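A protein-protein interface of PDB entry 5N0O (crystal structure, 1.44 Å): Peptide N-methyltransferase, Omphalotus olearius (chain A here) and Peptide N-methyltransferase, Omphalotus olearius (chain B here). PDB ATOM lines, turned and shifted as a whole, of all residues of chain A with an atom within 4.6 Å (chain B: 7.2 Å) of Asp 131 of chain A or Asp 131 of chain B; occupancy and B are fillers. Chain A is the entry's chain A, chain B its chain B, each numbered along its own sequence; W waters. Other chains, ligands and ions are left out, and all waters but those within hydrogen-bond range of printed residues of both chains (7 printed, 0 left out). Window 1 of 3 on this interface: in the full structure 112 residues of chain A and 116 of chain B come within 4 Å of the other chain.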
ATOM      1  N   HIS A  99     -18.991 -15.828 -29.327  1.00  0.00           N
ATOM      2  CA  HIS A  99     -19.759 -14.691 -29.884  1.00  0.00           C
ATOM      3  C   HIS A  99     -20.553 -15.278 -31.060  1.00  0.00           C
ATOM      4  O   HIS A  99     -19.968 -15.937 -31.936  1.00  0.00           O
ATOM      5  CB  HIS A  99     -18.763 -13.618 -30.364  1.00  0.00           C
ATOM      6  CG  HIS A  99     -19.368 -12.353 -30.939  1.00  0.00           C
ATOM      7  ND1 HIS A  99     -20.314 -12.335 -31.948  1.00  0.00           N
ATOM      8  CD2 HIS A  99     -19.051 -11.053 -30.709  1.00  0.00           C
ATOM      9  CE1 HIS A  99     -20.588 -11.078 -32.273  1.00  0.00           C
ATOM     10  NE2 HIS A  99     -19.820 -10.280 -31.552  1.00  0.00           N
ATOM     11  N   PRO A 125     -23.751  -9.289 -28.600  1.00  0.00           N
ATOM     12  CA  PRO A 125     -22.371  -9.787 -28.658  1.00  0.00           C
ATOM     13  C   PRO A 125     -22.016 -10.708 -27.481  1.00  0.00           C
ATOM     14  O   PRO A 125     -22.662 -10.654 -26.429  1.00  0.00           O
ATOM     15  CB  PRO A 125     -21.542  -8.500 -28.591  1.00  0.00           C
ATOM     16  CG  PRO A 125     -22.403  -7.588 -27.767  1.00  0.00           C
ATOM     17  CD  PRO A 125     -23.797  -7.861 -28.233  1.00  0.00           C
ATOM     18  N   GLY A 126     -21.002 -11.541 -27.672  1.00  0.00           N
ATOM     19  CA  GLY A 126     -20.452 -12.382 -26.605  1.00  0.00           C
ATOM     20  C   GLY A 126     -18.940 -12.483 -26.684  1.00  0.00           C
ATOM     21  O   GLY A 126     -18.304 -11.839 -27.531  1.00  0.00           O
ATOM     22  N   VAL A 127     -18.367 -13.287 -25.789  1.00  0.00           N
ATOM     23  CA  VAL A 127     -16.921 -13.477 -25.665  1.00  0.00           C
ATOM     24  C   VAL A 127     -16.445 -14.536 -26.667  1.00  0.00           C
ATOM     25  O   VAL A 127     -16.840 -15.705 -26.578  1.00  0.00           O
ATOM     26  CB  VAL A 127     -16.542 -13.876 -24.208  1.00  0.00           C
ATOM     27  CG1 VAL A 127     -15.053 -14.203 -24.099  1.00  0.00           C
ATOM     28  CG2 VAL A 127     -16.946 -12.776 -23.218  1.00  0.00           C
ATOM     29  N   SER A 128     -15.607 -14.136 -27.623  1.00  0.00           N
ATOM     30  CA  SER A 128     -15.127 -15.047 -28.680  1.00  0.00           C
ATOM     31  C   SER A 128     -13.847 -15.796 -28.302  1.00  0.00           C
ATOM     32  O   SER A 128     -13.163 -15.459 -27.320  1.00  0.00           O
ATOM     33  CB  SER A 128     -14.849 -14.266 -29.970  1.00  0.00           C
ATOM     34  OG  SER A 128     -13.608 -13.569 -29.883  1.00  0.00           O
ATOM     35  N   ALA A 129     -13.458 -16.765 -29.129  1.00  0.00           N
ATOM     36  CA  ALA A 129     -12.162 -17.428 -28.955  1.00  0.00           C
ATOM     37  C   ALA A 129     -10.973 -16.467 -29.122  1.00  0.00           C
ATOM     38  O   ALA A 129      -9.932 -16.681 -28.501  1.00  0.00           O
ATOM     39  CB  ALA A 129     -12.036 -18.623 -29.908  1.00  0.00           C
ATOM     40  N   GLU A 130     -11.128 -15.416 -29.944  1.00  0.00           N
ATOM     41  CA  GLU A 130     -10.083 -14.385 -30.062  1.00  0.00           C
ATOM     42  C   GLU A 130      -9.970 -13.550 -28.771  1.00  0.00           C
ATOM     43  O   GLU A 130      -8.849 -13.224 -28.330  1.00  0.00           O
ATOM     44  CB  GLU A 130     -10.288 -13.503 -31.304  1.00  0.00           C
ATOM     45  CG  GLU A 130      -9.140 -12.510 -31.473  1.00  0.00           C
ATOM     46  CD  GLU A 130      -9.102 -11.800 -32.814  1.00  0.00           C
ATOM     47  OE1 GLU A 130      -9.746 -10.742 -32.949  1.00  0.00           O
ATOM     48  OE2 GLU A 130      -8.370 -12.279 -33.718  1.00  0.00           O
ATOM     49  N   ASP A 131     -11.112 -13.215 -28.171  1.00  0.00           N
ATOM     50  CA  ASP A 131     -11.115 -12.550 -26.844  1.00  0.00           C
ATOM     51  C   ASP A 131     -10.345 -13.384 -25.803  1.00  0.00           C
ATOM     52  O   ASP A 131      -9.528 -12.846 -25.019  1.00  0.00           O
ATOM     53  CB  ASP A 131     -12.546 -12.293 -26.358  1.00  0.00           C
ATOM     54  CG  ASP A 131     -13.245 -11.191 -27.117  1.00  0.00           C
ATOM     55  OD1 ASP A 131     -12.582 -10.180 -27.486  1.00  0.00           O
ATOM     56  OD2 ASP A 131     -14.489 -11.320 -27.315  1.00  0.00           O
ATOM     57  N   CYS A 132     -10.584 -14.704 -25.803  1.00  0.00           N
ATOM     58  CA  CYS A 132      -9.848 -15.612 -24.899  1.00  0.00           C
ATOM     59  C   CYS A 132      -8.353 -15.651 -25.208  1.00  0.00           C
ATOM     60  O   CYS A 132      -7.508 -15.614 -24.282  1.00  0.00           O
ATOM     61  CB  CYS A 132     -10.455 -17.031 -24.943  1.00  0.00           C
ATOM     62  SG  CYS A 132     -12.175 -17.158 -24.344  1.00  0.00           S
ATOM     63  N   LEU A 133      -8.003 -15.693 -26.501  1.00  0.00           N
ATOM     64  CA  LEU A 133      -6.598 -15.705 -26.951  1.00  0.00           C
ATOM     65  C   LEU A 133      -5.833 -14.479 -26.400  1.00  0.00           C
ATOM     66  O   LEU A 133      -4.734 -14.624 -25.833  1.00  0.00           O
ATOM     67  CB  LEU A 133      -6.573 -15.762 -28.489  1.00  0.00           C
ATOM     68  CG  LEU A 133      -5.239 -15.895 -29.231  1.00  0.00           C
ATOM     69  CD1 LEU A 133      -5.470 -16.527 -30.611  1.00  0.00           C
ATOM     70  CD2 LEU A 133      -4.494 -14.568 -29.371  1.00  0.00           C
ATOM     71  N   PHE A 134      -6.419 -13.285 -26.538  1.00  0.00           N
ATOM     72  CA  PHE A 134      -5.763 -12.072 -26.001  1.00  0.00           C
ATOM     73  C   PHE A 134      -5.488 -12.204 -24.484  1.00  0.00           C
ATOM     74  O   PHE A 134      -4.382 -11.901 -24.006  1.00  0.00           O
ATOM     75  CB  PHE A 134      -6.589 -10.803 -26.256  1.00  0.00           C
ATOM     76  CG  PHE A 134      -6.845 -10.465 -27.719  1.00  0.00           C
ATOM     77  CD1 PHE A 134      -5.917 -10.729 -28.728  1.00  0.00           C
ATOM     78  CD2 PHE A 134      -8.036  -9.818 -28.071  1.00  0.00           C
ATOM     79  CE1 PHE A 134      -6.186 -10.374 -30.055  1.00  0.00           C
ATOM     80  CE2 PHE A 134      -8.300  -9.453 -29.380  1.00  0.00           C
ATOM     81  CZ  PHE A 134      -7.375  -9.728 -30.369  1.00  0.00           C
ATOM     82  N   ALA A 135      -6.489 -12.685 -23.737  1.00  0.00           N
ATOM     83  CA  ALA A 135      -6.372 -12.837 -22.275  1.00  0.00           C
ATOM     84  C   ALA A 135      -5.331 -13.888 -21.848  1.00  0.00           C
ATOM     85  O   ALA A 135      -4.539 -13.662 -20.919  1.00  0.00           O
ATOM     86  CB  ALA A 135      -7.739 -13.153 -21.674  1.00  0.00           C
ATOM     87  N   ILE B  18     -19.583  -3.407 -22.733  1.00  0.00           N
ATOM     88  CA  ILE B  18     -19.782  -1.998 -23.163  1.00  0.00           C
ATOM     89  C   ILE B  18     -21.132  -1.441 -22.688  1.00  0.00           C
ATOM     90  O   ILE B  18     -21.199  -0.353 -22.094  1.00  0.00           O
ATOM     91  CB  ILE B  18     -19.621  -1.853 -24.705  1.00  0.00           C
ATOM     92  CG1 ILE B  18     -18.202  -2.263 -25.146  1.00  0.00           C
ATOM     93  CG2 ILE B  18     -19.955  -0.438 -25.175  1.00  0.00           C
ATOM     94  CD1 ILE B  18     -17.076  -1.351 -24.658  1.00  0.00           C
ATOM     95  N   HIS B  99     -13.537  -5.397 -22.744  1.00  0.00           N
ATOM     96  CA  HIS B  99     -12.538  -6.457 -22.506  1.00  0.00           C
ATOM     97  C   HIS B  99     -11.330  -5.763 -21.869  1.00  0.00           C
ATOM     98  O   HIS B  99     -10.834  -4.750 -22.414  1.00  0.00           O
ATOM     99  CB  HIS B  99     -12.168  -7.114 -23.849  1.00  0.00           C
ATOM    100  CG  HIS B  99     -11.192  -8.260 -23.783  1.00  0.00           C
ATOM    101  ND1 HIS B  99      -9.970  -8.197 -23.135  1.00  0.00           N
ATOM    102  CD2 HIS B  99     -11.233  -9.478 -24.380  1.00  0.00           C
ATOM    103  CE1 HIS B  99      -9.314  -9.335 -23.333  1.00  0.00           C
ATOM    104  NE2 HIS B  99     -10.062 -10.131 -24.084  1.00  0.00           N
ATOM    105  N   VAL B 102      -8.073  -5.192 -24.228  1.00  0.00           N
ATOM    106  CA  VAL B 102      -8.255  -4.730 -25.619  1.00  0.00           C
ATOM    107  C   VAL B 102      -8.176  -3.204 -25.586  1.00  0.00           C
ATOM    108  O   VAL B 102      -9.089  -2.536 -25.090  1.00  0.00           O
ATOM    109  CB  VAL B 102      -9.590  -5.274 -26.200  1.00  0.00           C
ATOM    110  CG1 VAL B 102      -9.996  -4.599 -27.508  1.00  0.00           C
ATOM    111  CG2 VAL B 102      -9.476  -6.781 -26.404  1.00  0.00           C
ATOM    112  N   MET B 123      -6.009 -12.926 -16.442  1.00  0.00           N
ATOM    113  CA  MET B 123      -7.016 -12.074 -17.081  1.00  0.00           C
ATOM    114  C   MET B 123      -8.194 -12.913 -17.505  1.00  0.00           C
ATOM    115  O   MET B 123      -8.019 -13.992 -18.108  1.00  0.00           O
ATOM    116  CB  MET B 123      -6.458 -11.372 -18.321  1.00  0.00           C
ATOM    117  CG  MET B 123      -7.450 -10.318 -18.831  1.00  0.00           C
ATOM    118  SD  MET B 123      -6.757  -9.408 -20.422  1.00  0.00           S
ATOM    119  CE  MET B 123      -5.529  -8.124 -19.564  1.00  0.00           C
ATOM    120  N   LEU B 124      -9.403 -12.434 -17.194  1.00  0.00           N
ATOM    121  CA  LEU B 124     -10.657 -13.044 -17.693  1.00  0.00           C
ATOM    122  C   LEU B 124     -11.200 -12.162 -18.829  1.00  0.00           C
ATOM    123  O   LEU B 124     -11.370 -10.952 -18.648  1.00  0.00           O
ATOM    124  CB  LEU B 124     -11.714 -13.181 -16.576  1.00  0.00           C
ATOM    125  CG  LEU B 124     -11.316 -13.929 -15.296  1.00  0.00           C
ATOM    126  CD1 LEU B 124     -12.502 -14.097 -14.357  1.00  0.00           C
ATOM    127  CD2 LEU B 124     -10.700 -15.280 -15.615  1.00  0.00           C
ATOM    128  N   PRO B 125     -11.466 -12.750 -20.013  1.00  0.00           N
ATOM    129  CA  PRO B 125     -11.924 -11.947 -21.162  1.00  0.00           C
ATOM    130  C   PRO B 125     -13.328 -11.336 -20.978  1.00  0.00           C
ATOM    131  O   PRO B 125     -14.126 -11.854 -20.178  1.00  0.00           O
ATOM    132  CB  PRO B 125     -11.912 -12.976 -22.304  1.00  0.00           C
ATOM    133  CG  PRO B 125     -12.245 -14.256 -21.609  1.00  0.00           C
ATOM    134  CD  PRO B 125     -11.435 -14.191 -20.349  1.00  0.00           C
ATOM    135  N   GLY B 126     -13.620 -10.259 -21.711  1.00  0.00           N
ATOM    136  CA  GLY B 126     -14.942  -9.636 -21.750  1.00  0.00           C
ATOM    137  C   GLY B 126     -15.337  -9.248 -23.164  1.00  0.00           C
ATOM    138  O   GLY B 126     -14.591  -9.504 -24.129  1.00  0.00           O
ATOM    139  N   VAL B 127     -16.525  -8.647 -23.271  1.00  0.00           N
ATOM    140  CA  VAL B 127     -17.109  -8.184 -24.539  1.00  0.00           C
ATOM    141  C   VAL B 127     -16.516  -6.801 -24.898  1.00  0.00           C
ATOM    142  O   VAL B 127     -16.726  -5.828 -24.171  1.00  0.00           O
ATOM    143  CB  VAL B 127     -18.654  -8.105 -24.426  1.00  0.00           C
ATOM    144  CG1 VAL B 127     -19.274  -7.470 -25.676  1.00  0.00           C
ATOM    145  CG2 VAL B 127     -19.240  -9.500 -24.165  1.00  0.00           C
ATOM    146  N   SER B 128     -15.781  -6.724 -26.013  1.00  0.00           N
ATOM    147  CA  SER B 128     -15.119  -5.477 -26.450  1.00  0.00           C
ATOM    148  C   SER B 128     -16.001  -4.611 -27.355  1.00  0.00           C
ATOM    149  O   SER B 128     -17.057  -5.056 -27.848  1.00  0.00           O
ATOM    150  CB  SER B 128     -13.830  -5.803 -27.216  1.00  0.00           C
ATOM    151  OG  SER B 128     -14.113  -6.216 -28.564  1.00  0.00           O
ATOM    152  N   ALA B 129     -15.549  -3.386 -27.628  1.00  0.00           N
ATOM    153  CA  ALA B 129     -16.256  -2.526 -28.597  1.00  0.00           C
ATOM    154  C   ALA B 129     -16.271  -3.126 -30.009  1.00  0.00           C
ATOM    155  O   ALA B 129     -17.221  -2.887 -30.771  1.00  0.00           O
ATOM    156  CB  ALA B 129     -15.666  -1.114 -28.614  1.00  0.00           C
ATOM    157  N   GLU B 130     -15.238  -3.908 -30.358  1.00  0.00           N
ATOM    158  CA  GLU B 130     -15.208  -4.597 -31.659  1.00  0.00           C
ATOM    159  C   GLU B 130     -16.248  -5.725 -31.711  1.00  0.00           C
ATOM    160  O   GLU B 130     -16.888  -5.924 -32.745  1.00  0.00           O
ATOM    161  CB  GLU B 130     -13.805  -5.123 -32.000  1.00  0.00           C
ATOM    162  CG  GLU B 130     -13.752  -5.788 -33.380  1.00  0.00           C
ATOM    163  CD  GLU B 130     -12.353  -6.084 -33.895  1.00  0.00           C
ATOM    164  OE1 GLU B 130     -11.799  -7.165 -33.610  1.00  0.00           O
ATOM    165  OE2 GLU B 130     -11.822  -5.248 -34.652  1.00  0.00           O
ATOM    166  N   ASP B 131     -16.421  -6.453 -30.603  1.00  0.00           N
ATOM    167  CA  ASP B 131     -17.492  -7.468 -30.505  1.00  0.00           C
ATOM    168  C   ASP B 131     -18.869  -6.827 -30.740  1.00  0.00           C
ATOM    169  O   ASP B 131     -19.707  -7.377 -31.465  1.00  0.00           O
ATOM    170  CB  ASP B 131     -17.470  -8.154 -29.122  1.00  0.00           C
ATOM    171  CG  ASP B 131     -16.312  -9.136 -28.949  1.00  0.00           C
ATOM    172  OD1 ASP B 131     -15.962  -9.840 -29.922  1.00  0.00           O
ATOM    173  OD2 ASP B 131     -15.769  -9.245 -27.807  1.00  0.00           O
ATOM    174  N   CYS B 132     -19.100  -5.666 -30.116  1.00  0.00           N
ATOM    175  CA  CYS B 132     -20.346  -4.910 -30.316  1.00  0.00           C
ATOM    176  C   CYS B 132     -20.497  -4.473 -31.781  1.00  0.00           C
ATOM    177  O   CYS B 132     -21.592  -4.578 -32.366  1.00  0.00           O
ATOM    178  CB  CYS B 132     -20.403  -3.690 -29.381  1.00  0.00           C
ATOM    179  SG  CYS B 132     -20.491  -4.088 -27.614  1.00  0.00           S
ATOM    180  N   LEU B 133     -19.400  -3.992 -32.370  1.00  0.00           N
ATOM    181  CA  LEU B 133     -19.400  -3.542 -33.772  1.00  0.00           C
ATOM    182  C   LEU B 133     -19.853  -4.660 -34.728  1.00  0.00           C
ATOM    183  O   LEU B 133     -20.733  -4.440 -35.577  1.00  0.00           O
ATOM    184  CB  LEU B 133     -18.011  -2.998 -34.134  1.00  0.00           C
ATOM    185  CG  LEU B 133     -17.762  -2.376 -35.523  1.00  0.00           C
ATOM    186  CD1 LEU B 133     -16.550  -1.449 -35.470  1.00  0.00           C
ATOM    187  CD2 LEU B 133     -17.572  -3.417 -36.620  1.00  0.00           C
ATOM    188  N   PHE B 134     -19.289  -5.863 -34.580  1.00  0.00           N
ATOM    189  CA  PHE B 134     -19.710  -6.994 -35.419  1.00  0.00           C
ATOM    190  C   PHE B 134     -21.228  -7.245 -35.303  1.00  0.00           C
ATOM    191  O   PHE B 134     -21.928  -7.433 -36.314  1.00  0.00           O
ATOM    192  CB  PHE B 134     -18.951  -8.293 -35.059  1.00  0.00           C
ATOM    193  CG  PHE B 134     -17.436  -8.242 -35.241  1.00  0.00           C
ATOM    194  CD1 PHE B 134     -16.817  -7.501 -36.250  1.00  0.00           C
ATOM    195  CD2 PHE B 134     -16.625  -9.011 -34.397  1.00  0.00           C
ATOM    196  CE1 PHE B 134     -15.428  -7.512 -36.403  1.00  0.00           C
ATOM    197  CE2 PHE B 134     -15.247  -9.023 -34.548  1.00  0.00           C
ATOM    198  CZ  PHE B 134     -14.650  -8.282 -35.556  1.00  0.00           C
ATOM    199  N   ALA B 135     -21.740  -7.249 -34.067  1.00  0.00           N
ATOM    200  CA  ALA B 135     -23.169  -7.509 -33.806  1.00  0.00           C
ATOM    201  C   ALA B 135     -24.103  -6.420 -34.370  1.00  0.00           C
ATOM    202  O   ALA B 135     -25.142  -6.734 -34.955  1.00  0.00           O
ATOM    203  CB  ALA B 135     -23.420  -7.704 -32.312  1.00  0.00           C
ATOM    204  N   ASP B 136     -23.734  -5.155 -34.200  1.00  0.00           N
ATOM    205  CA  ASP B 136     -24.598  -4.023 -34.595  1.00  0.00           C
ATOM    206  C   ASP B 136     -24.523  -3.690 -36.089  1.00  0.00           C
ATOM    207  O   ASP B 136     -25.529  -3.262 -36.671  1.00  0.00           O
ATOM    208  CB  ASP B 136     -24.257  -2.758 -33.776  1.00  0.00           C
ATOM    209  CG  ASP B 136     -24.773  -2.805 -32.335  1.00  0.00           C
ATOM    210  OD1 ASP B 136     -25.769  -3.507 -32.038  1.00  0.00           O
ATOM    211  OD2 ASP B 136     -24.166  -2.106 -31.494  1.00  0.00           O
ATOM    212  N   ILE B 139     -21.798  -7.803 -39.498  1.00  0.00           N
ATOM    213  CA  ILE B 139     -20.652  -8.326 -40.253  1.00  0.00           C
ATOM    214  C   ILE B 139     -19.977  -9.435 -39.439  1.00  0.00           C
ATOM    215  O   ILE B 139     -20.100  -9.491 -38.205  1.00  0.00           O
ATOM    216  CB  ILE B 139     -19.625  -7.221 -40.640  1.00  0.00           C
ATOM    217  CG1 ILE B 139     -18.988  -6.556 -39.403  1.00  0.00           C
ATOM    218  CG2 ILE B 139     -20.268  -6.171 -41.552  1.00  0.00           C
ATOM    219  CD1 ILE B 139     -17.839  -5.610 -39.720  1.00  0.00           C
ATOM    220  N   PHE B 170      -9.685   2.025 -33.799  1.00  0.00           N
ATOM    221  CA  PHE B 170     -10.003   2.534 -32.449  1.00  0.00           C
ATOM    222  C   PHE B 170      -9.321   3.891 -32.228  1.00  0.00           C
ATOM    223  O   PHE B 170      -8.309   4.205 -32.870  1.00  0.00           O
ATOM    224  CB  PHE B 170      -9.494   1.564 -31.349  1.00  0.00           C
ATOM    225  CG  PHE B 170     -10.370   0.352 -31.079  1.00  0.00           C
ATOM    226  CD1 PHE B 170     -10.595  -0.616 -32.047  1.00  0.00           C
ATOM    227  CD2 PHE B 170     -10.896   0.142 -29.799  1.00  0.00           C
ATOM    228  CE1 PHE B 170     -11.360  -1.747 -31.759  1.00  0.00           C
ATOM    229  CE2 PHE B 170     -11.659  -0.981 -29.506  1.00  0.00           C
ATOM    230  CZ  PHE B 170     -11.890  -1.936 -30.490  1.00  0.00           C
ATOM    231  N   TYR B 210     -19.134   4.570 -35.770  1.00  0.00           N
ATOM    232  CA  TYR B 210     -19.794   3.635 -34.848  1.00  0.00           C
ATOM    233  C   TYR B 210     -19.622   4.016 -33.373  1.00  0.00           C
ATOM    234  O   TYR B 210     -18.494   4.174 -32.896  1.00  0.00           O
ATOM    235  CB  TYR B 210     -19.268   2.210 -35.069  1.00  0.00           C
ATOM    236  CG  TYR B 210     -19.894   1.190 -34.116  1.00  0.00           C
ATOM    237  CD1 TYR B 210     -21.266   0.918 -34.156  1.00  0.00           C
ATOM    238  CD2 TYR B 210     -19.127   0.534 -33.154  1.00  0.00           C
ATOM    239  CE1 TYR B 210     -21.849   0.000 -33.289  1.00  0.00           C
ATOM    240  CE2 TYR B 210     -19.702  -0.384 -32.282  1.00  0.00           C
ATOM    241  CZ  TYR B 210     -21.062  -0.636 -32.340  1.00  0.00           C
ATOM    242  OH  TYR B 210     -21.640  -1.559 -31.481  1.00  0.00           O
HETATM  243  O   HOH W   1      -5.517  -9.162 -23.462  1.00  0.00           O
HETATM  244  O   HOH W   2     -11.042  -9.631 -35.466  1.00  0.00           O
HETATM  245  O   HOH W   3      -8.817  -7.817 -33.457  1.00  0.00           O
HETATM  246  O   HOH W   4      -4.271 -14.612 -18.194  1.00  0.00           O
HETATM  247  O   HOH W   5     -11.901  -9.249 -31.779  1.00  0.00           O
HETATM  248  O   HOH W   6     -12.306  -8.059 -29.190  1.00  0.00           O
HETATM  249  O   HOH W   7     -13.953 -11.221 -31.165  1.00  0.00           O
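O of Asp 131 of chain B lies within hydrogen-bond range of NE2 of His 99 of chain A (2.9 Å).
O of Asp 131 of chain A lies within hydrogen-bond range of NE2 of His 99 of chain B, at 2.9 Å.
The side-chain carboxylate (OD2) of Asp 131 of chain A sits close to the side-chain carboxylate (OD2) of Asp 131 of chain B.
The backbone carbonyl oxygen of Val 127 of chain A sits at hydrogen-bond distance from the backbone NH of His 99 of chain A (3.5 Å).
N of Ser 128 of chain A sits at hydrogen-bond distance from OD2 of Asp 131 of chain A.
O of Ser 128 of chain A sits at hydrogen-bond distance from SG of Cys 132 of chain A, 3.6 Å away.
N of Asp 131 of chain B is in hydrogen-bond range of OG of Ser 128 of chain B, 3.1 Å away.
O of Ser 128 of chain B lies within hydrogen-bond range of SG of Cys 132 of chain B (3.6 Å).
The backbone carbonyl oxygen (O) of Cys 132 of chain B sits close to the side-chain hydroxyl (OH) of Tyr 210 of chain B.
Among the printed residues, pairs that only touch across the chains: Pro 125 of chain A with Val 127 of chain B, Pro 125 of chain A with Asp 131 of chain B, Pro 125 of chain A with Cys 132 of chain B, Gly 126 of chain A with Val 127 of chain B, Gly 126 of chain A with Asp 131 of chain B, Val 127 of chain A with Pro 125 of chain B, Val 127 of chain A with Gly 126 of chain B, Asp 131 of chain A with Pro 125 of chain B, Asp 131 of chain A with Gly 126 of chain B, Cys 132 of chain A with Pro 125 of chain B, Phe 134 of chain A with Val 102 of chain B and Ala 135 of chain A with Met 123 of chain B.
Of the printed residues of chain A, His 99 of chain B touches Asp 131 (2.9 Å).
Printed residues of chain B within 4 Å of Val 127 of chain A: Pro 125 and Gly 126.
Printed residues of chain A within 4 Å of Pro 125 of chain B: Val 127, Asp 131 and Cys 132.
Printed residues of chain B within 4 Å of Pro 125 of chain A: Val 127, Asp 131 and Cys 132.
Phe 170 of chain B touches none of the printed residues of chain A.
The nearest residue of chain B that does not touch Asp 131 of chain A is Ser 128 of chain B (4.4 Å).
The nearest printed residue of chain A that does not touch Cys 132 of chain B is His 99 of chain A (4.9 Å).
Of the 20 printed residues of chain B, 8 touch a printed residue of chain A.
Hydrophobic or aromatic side chains of chain B within 4 Å of the printed part of chain A: His 99, Val 102, Met 123, Pro 125 and Val 127.
Of the 12 printed residues of chain A, 8 touch a printed residue of chain B.
Hydrophobic or aromatic side chains of chain A that line the printed part of chain B: His 99, Pro 125, Val 127, Phe 134 and Ala 135.
Along chain A the printed residues that touch a printed residue of chain B span positions 99 to 135.
Water W6 lies within hydrogen-bond range of OG of Ser 128 of chain B (2.7 Å) and OD1 of Asp 131 of chain A (2.7 Å).
Water W7 lies within hydrogen-bond range of the side-chain hydroxyl of Ser 128 of chain A (2.7 Å) and the side-chain carboxylate of Asp 131 of chain B (2.7 Å).
Water W5 bridges the side-chain carboxylate of Glu 130 of chain B (2.8 Å) and the side-chain carboxylate of Glu 130 of chain A (2.9 Å).
Water W4 bridges the backbone carbonyl oxygen (O) of Ala 135 of chain A (2.9 Å) and the backbone NH (N) of Met 123 of chain B (3.0 Å).
Water W1 bridges O of Phe 134 of chain A (3.0 Å) and SD of Met 123 of chain B (3.3 Å).
Water W2 bridges OE1 of Glu 130 of chain A (3.0 Å) and OE1 of Glu 130 of chain B (3.2 Å).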
